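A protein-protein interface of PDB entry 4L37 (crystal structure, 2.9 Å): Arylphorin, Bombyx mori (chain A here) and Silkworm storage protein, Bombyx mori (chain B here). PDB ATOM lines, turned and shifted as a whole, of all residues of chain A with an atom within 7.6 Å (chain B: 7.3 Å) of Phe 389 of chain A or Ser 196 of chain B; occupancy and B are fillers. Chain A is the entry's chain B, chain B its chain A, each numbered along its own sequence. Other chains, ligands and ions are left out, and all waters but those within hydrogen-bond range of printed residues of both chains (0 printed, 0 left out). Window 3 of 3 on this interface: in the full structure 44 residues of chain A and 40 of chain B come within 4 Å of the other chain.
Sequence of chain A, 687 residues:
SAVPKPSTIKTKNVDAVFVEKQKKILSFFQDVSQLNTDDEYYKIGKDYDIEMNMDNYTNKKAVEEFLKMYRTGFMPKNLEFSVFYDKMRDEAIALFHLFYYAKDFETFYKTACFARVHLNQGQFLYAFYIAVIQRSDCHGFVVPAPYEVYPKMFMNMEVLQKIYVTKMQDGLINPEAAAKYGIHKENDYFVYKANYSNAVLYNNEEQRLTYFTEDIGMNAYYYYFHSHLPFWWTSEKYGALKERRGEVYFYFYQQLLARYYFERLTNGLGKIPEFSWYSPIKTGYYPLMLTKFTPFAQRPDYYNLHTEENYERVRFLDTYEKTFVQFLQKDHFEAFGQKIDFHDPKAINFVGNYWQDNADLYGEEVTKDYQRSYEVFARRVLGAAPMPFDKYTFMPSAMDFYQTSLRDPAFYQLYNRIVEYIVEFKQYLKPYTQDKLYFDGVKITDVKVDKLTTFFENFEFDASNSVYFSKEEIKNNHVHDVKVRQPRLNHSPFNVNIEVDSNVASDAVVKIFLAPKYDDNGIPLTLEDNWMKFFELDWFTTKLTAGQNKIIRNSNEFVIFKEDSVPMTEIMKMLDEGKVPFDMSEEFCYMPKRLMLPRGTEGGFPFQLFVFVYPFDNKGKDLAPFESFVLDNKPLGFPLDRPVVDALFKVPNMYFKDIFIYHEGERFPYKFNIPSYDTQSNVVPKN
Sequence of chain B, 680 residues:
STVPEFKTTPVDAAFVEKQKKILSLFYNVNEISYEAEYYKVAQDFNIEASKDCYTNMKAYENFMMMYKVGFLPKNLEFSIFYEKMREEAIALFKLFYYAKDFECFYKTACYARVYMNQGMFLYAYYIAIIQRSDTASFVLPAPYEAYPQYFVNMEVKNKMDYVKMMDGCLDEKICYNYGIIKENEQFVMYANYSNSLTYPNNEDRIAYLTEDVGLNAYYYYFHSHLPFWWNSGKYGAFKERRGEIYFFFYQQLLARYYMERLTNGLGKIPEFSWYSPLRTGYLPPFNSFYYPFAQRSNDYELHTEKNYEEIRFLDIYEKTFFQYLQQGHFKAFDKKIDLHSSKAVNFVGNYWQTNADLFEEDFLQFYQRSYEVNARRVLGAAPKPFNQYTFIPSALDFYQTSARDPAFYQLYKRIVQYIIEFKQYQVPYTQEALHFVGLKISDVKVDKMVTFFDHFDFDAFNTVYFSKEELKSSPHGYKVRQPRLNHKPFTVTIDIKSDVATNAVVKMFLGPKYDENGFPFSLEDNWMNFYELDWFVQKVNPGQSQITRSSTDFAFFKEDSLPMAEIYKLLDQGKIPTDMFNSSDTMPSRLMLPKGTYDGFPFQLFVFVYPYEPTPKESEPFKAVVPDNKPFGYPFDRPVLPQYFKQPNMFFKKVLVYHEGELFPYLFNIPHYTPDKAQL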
ATOM      1  N   PRO A 386       2.758  21.822  23.923  1.00  0.00           N
ATOM      2  CA  PRO A 386       3.802  22.047  22.928  1.00  0.00           C
ATOM      3  C   PRO A 386       4.677  20.791  22.828  1.00  0.00           C
ATOM      4  O   PRO A 386       4.624  19.955  23.741  1.00  0.00           O
ATOM      5  CB  PRO A 386       4.597  23.203  23.531  1.00  0.00           C
ATOM      6  CG  PRO A 386       4.422  23.027  24.980  1.00  0.00           C
ATOM      7  CD  PRO A 386       3.003  22.572  25.154  1.00  0.00           C
ATOM      8  N   MET A 387       5.477  20.661  21.762  1.00  0.00           N
ATOM      9  CA  MET A 387       6.314  19.468  21.518  1.00  0.00           C
ATOM     10  C   MET A 387       7.281  19.223  22.646  1.00  0.00           C
ATOM     11  O   MET A 387       7.900  20.156  23.163  1.00  0.00           O
ATOM     12  CB  MET A 387       7.091  19.595  20.235  1.00  0.00           C
ATOM     13  CG  MET A 387       6.209  19.933  19.083  1.00  0.00           C
ATOM     14  SD  MET A 387       5.203  18.501  18.719  1.00  0.00           S
ATOM     15  CE  MET A 387       6.311  17.601  17.616  1.00  0.00           C
ATOM     16  N   PRO A 388       7.419  17.959  23.047  1.00  0.00           N
ATOM     17  CA  PRO A 388       8.302  17.658  24.165  1.00  0.00           C
ATOM     18  C   PRO A 388       9.712  18.169  23.879  1.00  0.00           C
ATOM     19  O   PRO A 388      10.135  18.149  22.716  1.00  0.00           O
ATOM     20  CB  PRO A 388       8.256  16.128  24.262  1.00  0.00           C
ATOM     21  CG  PRO A 388       7.527  15.653  23.041  1.00  0.00           C
ATOM     22  CD  PRO A 388       6.663  16.784  22.590  1.00  0.00           C
ATOM     23  N   PHE A 389      10.382  18.664  24.927  1.00  0.00           N
ATOM     24  CA  PHE A 389      11.756  19.138  24.867  1.00  0.00           C
ATOM     25  C   PHE A 389      12.680  18.015  24.420  1.00  0.00           C
ATOM     26  O   PHE A 389      13.218  18.083  23.338  1.00  0.00           O
ATOM     27  CB  PHE A 389      12.166  19.635  26.231  1.00  0.00           C
ATOM     28  CG  PHE A 389      13.522  20.242  26.269  1.00  0.00           C
ATOM     29  CD1 PHE A 389      13.808  21.401  25.540  1.00  0.00           C
ATOM     30  CD2 PHE A 389      14.509  19.708  27.086  1.00  0.00           C
ATOM     31  CE1 PHE A 389      15.074  22.004  25.603  1.00  0.00           C
ATOM     32  CE2 PHE A 389      15.778  20.303  27.153  1.00  0.00           C
ATOM     33  CZ  PHE A 389      16.063  21.447  26.409  1.00  0.00           C
ATOM     34  N   ASP A 390      12.846  16.990  25.266  1.00  0.00           N
ATOM     35  CA  ASP A 390      13.486  15.706  24.944  1.00  0.00           C
ATOM     36  C   ASP A 390      12.571  14.575  25.420  1.00  0.00           C
ATOM     37  O   ASP A 390      11.466  14.816  25.949  1.00  0.00           O
ATOM     38  CB  ASP A 390      14.882  15.592  25.593  1.00  0.00           C
ATOM     39  CG  ASP A 390      14.845  15.584  27.135  1.00  0.00           C
ATOM     40  OD1 ASP A 390      13.830  15.188  27.739  1.00  0.00           O
ATOM     41  OD2 ASP A 390      15.855  15.962  27.779  1.00  0.00           O
ATOM     42  N   LYS A 391      13.044  13.339  25.267  1.00  0.00           N
ATOM     43  CA  LYS A 391      12.252  12.123  25.566  1.00  0.00           C
ATOM     44  C   LYS A 391      11.739  12.047  27.011  1.00  0.00           C
ATOM     45  O   LYS A 391      10.677  11.519  27.266  1.00  0.00           O
ATOM     46  CB  LYS A 391      13.049  10.870  25.193  1.00  0.00           C
ATOM     47  CG  LYS A 391      14.548  11.060  25.404  1.00  0.00           C
ATOM     48  CD  LYS A 391      15.345   9.764  25.362  1.00  0.00           C
ATOM     49  CE  LYS A 391      16.828  10.030  25.607  1.00  0.00           C
ATOM     50  NZ  LYS A 391      17.549   8.796  26.021  1.00  0.00           N
ATOM     51  N   TYR A 392      12.488  12.569  27.965  1.00  0.00           N
ATOM     52  CA  TYR A 392      12.030  12.564  29.336  1.00  0.00           C
ATOM     53  C   TYR A 392      11.352  13.905  29.747  1.00  0.00           C
ATOM     54  O   TYR A 392      10.874  14.085  30.889  1.00  0.00           O
ATOM     55  CB  TYR A 392      13.216  12.293  30.223  1.00  0.00           C
ATOM     56  CG  TYR A 392      13.893  10.969  29.998  1.00  0.00           C
ATOM     57  CD1 TYR A 392      13.155   9.789  29.900  1.00  0.00           C
ATOM     58  CD2 TYR A 392      15.291  10.876  29.949  1.00  0.00           C
ATOM     59  CE1 TYR A 392      13.781   8.559  29.730  1.00  0.00           C
ATOM     60  CE2 TYR A 392      15.929   9.649  29.791  1.00  0.00           C
ATOM     61  CZ  TYR A 392      15.168   8.497  29.676  1.00  0.00           C
ATOM     62  OH  TYR A 392      15.784   7.285  29.496  1.00  0.00           O
ATOM     63  N   THR A 393      11.310  14.857  28.819  1.00  0.00           N
ATOM     64  CA  THR A 393      10.858  16.185  29.193  1.00  0.00           C
ATOM     65  C   THR A 393       9.756  16.659  28.266  1.00  0.00           C
ATOM     66  O   THR A 393       9.999  17.008  27.104  1.00  0.00           O
ATOM     67  CB  THR A 393      12.020  17.193  29.260  1.00  0.00           C
ATOM     68  OG1 THR A 393      13.161  16.562  29.857  1.00  0.00           O
ATOM     69  CG2 THR A 393      11.636  18.383  30.110  1.00  0.00           C
ATOM     70  N   PHE A 394       8.538  16.652  28.805  1.00  0.00           N
ATOM     71  CA  PHE A 394       7.357  17.023  28.054  1.00  0.00           C
ATOM     72  C   PHE A 394       6.422  17.865  28.945  1.00  0.00           C
ATOM     73  O   PHE A 394       6.536  17.833  30.187  1.00  0.00           O
ATOM     74  CB  PHE A 394       6.651  15.763  27.540  1.00  0.00           C
ATOM     75  CG  PHE A 394       6.009  14.943  28.627  1.00  0.00           C
ATOM     76  CD1 PHE A 394       6.774  14.169  29.490  1.00  0.00           C
ATOM     77  CD2 PHE A 394       4.611  14.946  28.789  1.00  0.00           C
ATOM     78  CE1 PHE A 394       6.173  13.412  30.487  1.00  0.00           C
ATOM     79  CE2 PHE A 394       3.999  14.195  29.800  1.00  0.00           C
ATOM     80  CZ  PHE A 394       4.788  13.435  30.661  1.00  0.00           C
ATOM     81  N   MET A 395       5.508  18.622  28.325  1.00  0.00           N
ATOM     82  CA  MET A 395       4.508  19.268  29.127  1.00  0.00           C
ATOM     83  C   MET A 395       3.307  18.348  29.289  1.00  0.00           C
ATOM     84  O   MET A 395       2.642  18.036  28.307  1.00  0.00           O
ATOM     85  CB  MET A 395       4.088  20.604  28.564  1.00  0.00           C
ATOM     86  CG  MET A 395       2.919  21.171  29.339  1.00  0.00           C
ATOM     87  SD  MET A 395       2.648  22.862  28.857  1.00  0.00           S
ATOM     88  CE  MET A 395       3.650  23.720  30.090  1.00  0.00           C
ATOM     89  N   SER B 194      14.378  29.769  30.576  1.00  0.00           N
ATOM     90  CA  SER B 194      13.353  28.797  30.208  1.00  0.00           C
ATOM     91  C   SER B 194      13.623  27.937  28.978  1.00  0.00           C
ATOM     92  O   SER B 194      14.279  28.346  28.044  1.00  0.00           O
ATOM     93  CB  SER B 194      12.025  29.514  30.048  1.00  0.00           C
ATOM     94  OG  SER B 194      11.617  30.037  31.297  1.00  0.00           O
ATOM     95  N   ASN B 195      13.088  26.727  29.016  1.00  0.00           N
ATOM     96  CA  ASN B 195      12.899  25.849  27.862  1.00  0.00           C
ATOM     97  C   ASN B 195      12.017  26.395  26.734  1.00  0.00           C
ATOM     98  O   ASN B 195      11.417  27.485  26.790  1.00  0.00           O
ATOM     99  CB  ASN B 195      12.130  24.614  28.333  1.00  0.00           C
ATOM    100  CG  ASN B 195      12.998  23.656  29.056  1.00  0.00           C
ATOM    101  OD1 ASN B 195      14.215  23.787  29.041  1.00  0.00           O
ATOM    102  ND2 ASN B 195      12.399  22.686  29.698  1.00  0.00           N
ATOM    103  N   SER B 196      11.907  25.546  25.724  1.00  0.00           N
ATOM    104  CA  SER B 196      10.937  25.683  24.681  1.00  0.00           C
ATOM    105  C   SER B 196       9.576  25.137  25.142  1.00  0.00           C
ATOM    106  O   SER B 196       8.614  25.119  24.381  1.00  0.00           O
ATOM    107  CB  SER B 196      11.455  24.982  23.436  1.00  0.00           C
ATOM    108  OG  SER B 196      11.877  23.669  23.775  1.00  0.00           O
ATOM    109  N   LEU B 197       9.466  24.732  26.395  1.00  0.00           N
ATOM    110  CA  LEU B 197       8.155  24.385  26.911  1.00  0.00           C
ATOM    111  C   LEU B 197       7.551  25.584  27.598  1.00  0.00           C
ATOM    112  O   LEU B 197       6.460  25.487  28.176  1.00  0.00           O
ATOM    113  CB  LEU B 197       8.236  23.222  27.905  1.00  0.00           C
ATOM    114  CG  LEU B 197       8.683  21.849  27.394  1.00  0.00           C
ATOM    115  CD1 LEU B 197       8.855  20.907  28.583  1.00  0.00           C
ATOM    116  CD2 LEU B 197       7.757  21.291  26.284  1.00  0.00           C
ATOM    117  N   THR B 198       8.293  26.699  27.609  1.00  0.00           N
ATOM    118  CA  THR B 198       7.726  28.005  28.034  1.00  0.00           C
ATOM    119  C   THR B 198       7.785  29.052  26.883  1.00  0.00           C
ATOM    120  O   THR B 198       6.823  29.772  26.643  1.00  0.00           O
ATOM    121  CB  THR B 198       8.266  28.518  29.405  1.00  0.00           C
ATOM    122  OG1 THR B 198       8.916  29.780  29.230  1.00  0.00           O
ATOM    123  CG2 THR B 198       9.170  27.485  30.084  1.00  0.00           C
ATOM    124  N   TYR B 199       8.911  29.094  26.173  1.00  0.00           N
ATOM    125  CA  TYR B 199       9.037  29.826  24.907  1.00  0.00           C
ATOM    126  C   TYR B 199       9.096  28.849  23.712  1.00  0.00           C
ATOM    127  O   TYR B 199      10.188  28.477  23.276  1.00  0.00           O
ATOM    128  CB  TYR B 199      10.287  30.722  24.902  1.00  0.00           C
ATOM    129  CG  TYR B 199      10.246  31.893  25.836  1.00  0.00           C
ATOM    130  CD1 TYR B 199       9.608  33.086  25.486  1.00  0.00           C
ATOM    131  CD2 TYR B 199      10.857  31.822  27.083  1.00  0.00           C
ATOM    132  CE1 TYR B 199       9.555  34.175  26.371  1.00  0.00           C
ATOM    133  CE2 TYR B 199      10.819  32.912  27.970  1.00  0.00           C
ATOM    134  CZ  TYR B 199      10.178  34.087  27.600  1.00  0.00           C
ATOM    135  OH  TYR B 199      10.161  35.133  28.488  1.00  0.00           O
ATOM    136  N   PRO B 200       7.928  28.435  23.170  1.00  0.00           N
ATOM    137  CA  PRO B 200       7.917  27.300  22.207  1.00  0.00           C
ATOM    138  C   PRO B 200       8.162  27.697  20.742  1.00  0.00           C
ATOM    139  O   PRO B 200       7.430  27.276  19.846  1.00  0.00           O
ATOM    140  CB  PRO B 200       6.495  26.752  22.369  1.00  0.00           C
ATOM    141  CG  PRO B 200       5.696  27.992  22.586  1.00  0.00           C
ATOM    142  CD  PRO B 200       6.557  28.910  23.444  1.00  0.00           C
ATOM    143  N   ASN B 201       9.180  28.520  20.528  1.00  0.00           N
ATOM    144  CA  ASN B 201       9.540  29.039  19.215  1.00  0.00           C
ATOM    145  C   ASN B 201      10.924  29.704  19.337  1.00  0.00           C
ATOM    146  O   ASN B 201      11.562  29.647  20.412  1.00  0.00           O
ATOM    147  CB  ASN B 201       8.478  30.001  18.702  1.00  0.00           C
ATOM    148  CG  ASN B 201       7.964  30.920  19.797  1.00  0.00           C
ATOM    149  OD1 ASN B 201       8.759  31.623  20.408  1.00  0.00           O
ATOM    150  ND2 ASN B 201       6.638  30.899  20.077  1.00  0.00           N
ATOM    151  N   ASP B 204      12.710  31.827  22.385  1.00  0.00           N
ATOM    152  CA  ASP B 204      13.548  31.285  23.413  1.00  0.00           C
ATOM    153  C   ASP B 204      14.995  31.710  23.324  1.00  0.00           C
ATOM    154  O   ASP B 204      15.682  31.840  24.348  1.00  0.00           O
ATOM    155  CB  ASP B 204      13.503  29.782  23.334  1.00  0.00           C
ATOM    156  CG  ASP B 204      13.935  29.135  24.616  1.00  0.00           C
ATOM    157  OD1 ASP B 204      13.696  29.722  25.721  1.00  0.00           O
ATOM    158  OD2 ASP B 204      14.512  28.026  24.517  1.00  0.00           O
ATOM    159  N   LEU B 283       4.099  30.370  27.317  1.00  0.00           N
ATOM    160  CA  LEU B 283       3.527  29.619  28.379  1.00  0.00           C
ATOM    161  C   LEU B 283       4.129  30.130  29.652  1.00  0.00           C
ATOM    162  O   LEU B 283       5.251  29.772  29.988  1.00  0.00           O
ATOM    163  CB  LEU B 283       3.858  28.157  28.132  1.00  0.00           C
ATOM    164  CG  LEU B 283       2.862  27.553  27.100  1.00  0.00           C
ATOM    165  CD1 LEU B 283       3.282  27.592  25.636  1.00  0.00           C
ATOM    166  CD2 LEU B 283       2.513  26.117  27.468  1.00  0.00           C
ATOM    167  N   ASN B 298       1.199  28.688  20.298  1.00  0.00           N
ATOM    168  CA  ASN B 298       1.461  29.229  18.956  1.00  0.00           C
ATOM    169  C   ASN B 298       0.187  29.189  18.115  1.00  0.00           C
ATOM    170  O   ASN B 298      -0.639  28.307  18.285  1.00  0.00           O
ATOM    171  CB  ASN B 298       2.555  28.464  18.228  1.00  0.00           C
ATOM    172  CG  ASN B 298       3.850  28.374  19.018  1.00  0.00           C
ATOM    173  OD1 ASN B 298       4.332  29.339  19.637  1.00  0.00           O
ATOM    174  ND2 ASN B 298       4.428  27.200  18.995  1.00  0.00           N
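Of chain B, only Asn 195, Ser 196 and Leu 197 come within 4 Å of Phe 389 of chain A. Of the printed residues of chain A, Ser 196 of chain B touches Phe 389. Of the printed residues of chain A, Leu 197 of chain B touches Pro 386 (3.98 Å), Met 387 (3.3 Å), Phe 389 (3.95 Å), Phe 394 (3.9 Å) and Met 395 (3.8 Å). Printed residues of chain B within 4 Å of Pro 386 of chain A: Leu 197. Of the printed residues of chain B, Met 387 of chain A touches Leu 197 (3.3 Å). Of the printed residues of chain A, Asn 195 of chain B touches Phe 389 (3.97 Å). Pro 200 of chain B touches none of the printed residues of chain A. The nearest residue of chain B that does not touch Phe 389 of chain A is Asp 204 of chain B (6.1 Å). The nearest residue of chain A that does not touch Ser 196 of chain B is Pro 386 of chain A (4.5 Å).
The backbone carbonyl oxygen of Thr 198 of chain B is in hydrogen-bond range of the backbone NH of Leu 283 of chain B, 2.9 Å away.
Leu 197 of chain B touches Pro 386 of chain A (CD2 to CG, 3.98 Å). Leu 197 of chain B touches Met 387 of chain A. Asn 195 of chain B touches Phe 389 of chain A. Phe 389 of chain A touches Ser 196 of chain B. Phe 389 of chain A touches Leu 197 of chain B. CD1 of Leu 197 of chain B touches C of Phe 394 of chain A, at 3.9 Å. Leu 197 of chain B touches Met 395 of chain A. Leu 283 of chain B touches Met 395 of chain A (CD2 to SD, 3.5 Å).
Printed residues of chain B that touch a printed residue of chain A: Asn 195, Ser 196, Leu 197 and Leu 283. Hydrophobic or aromatic side chains of chain B within 4 Å of the printed part of chain A: Leu 197 and Leu 283. Along chain B the printed residues that touch a printed residue of chain A span positions 195 to 283. Of the 10 printed residues of chain A, 5 touch a printed residue of chain B. Among the printed residues, 8 pairs touch across the chains. Among the printed residues, no Asp or Glu carboxylate lies within 4 Å of a Lys or Arg side-chain nitrogen of the other chain.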
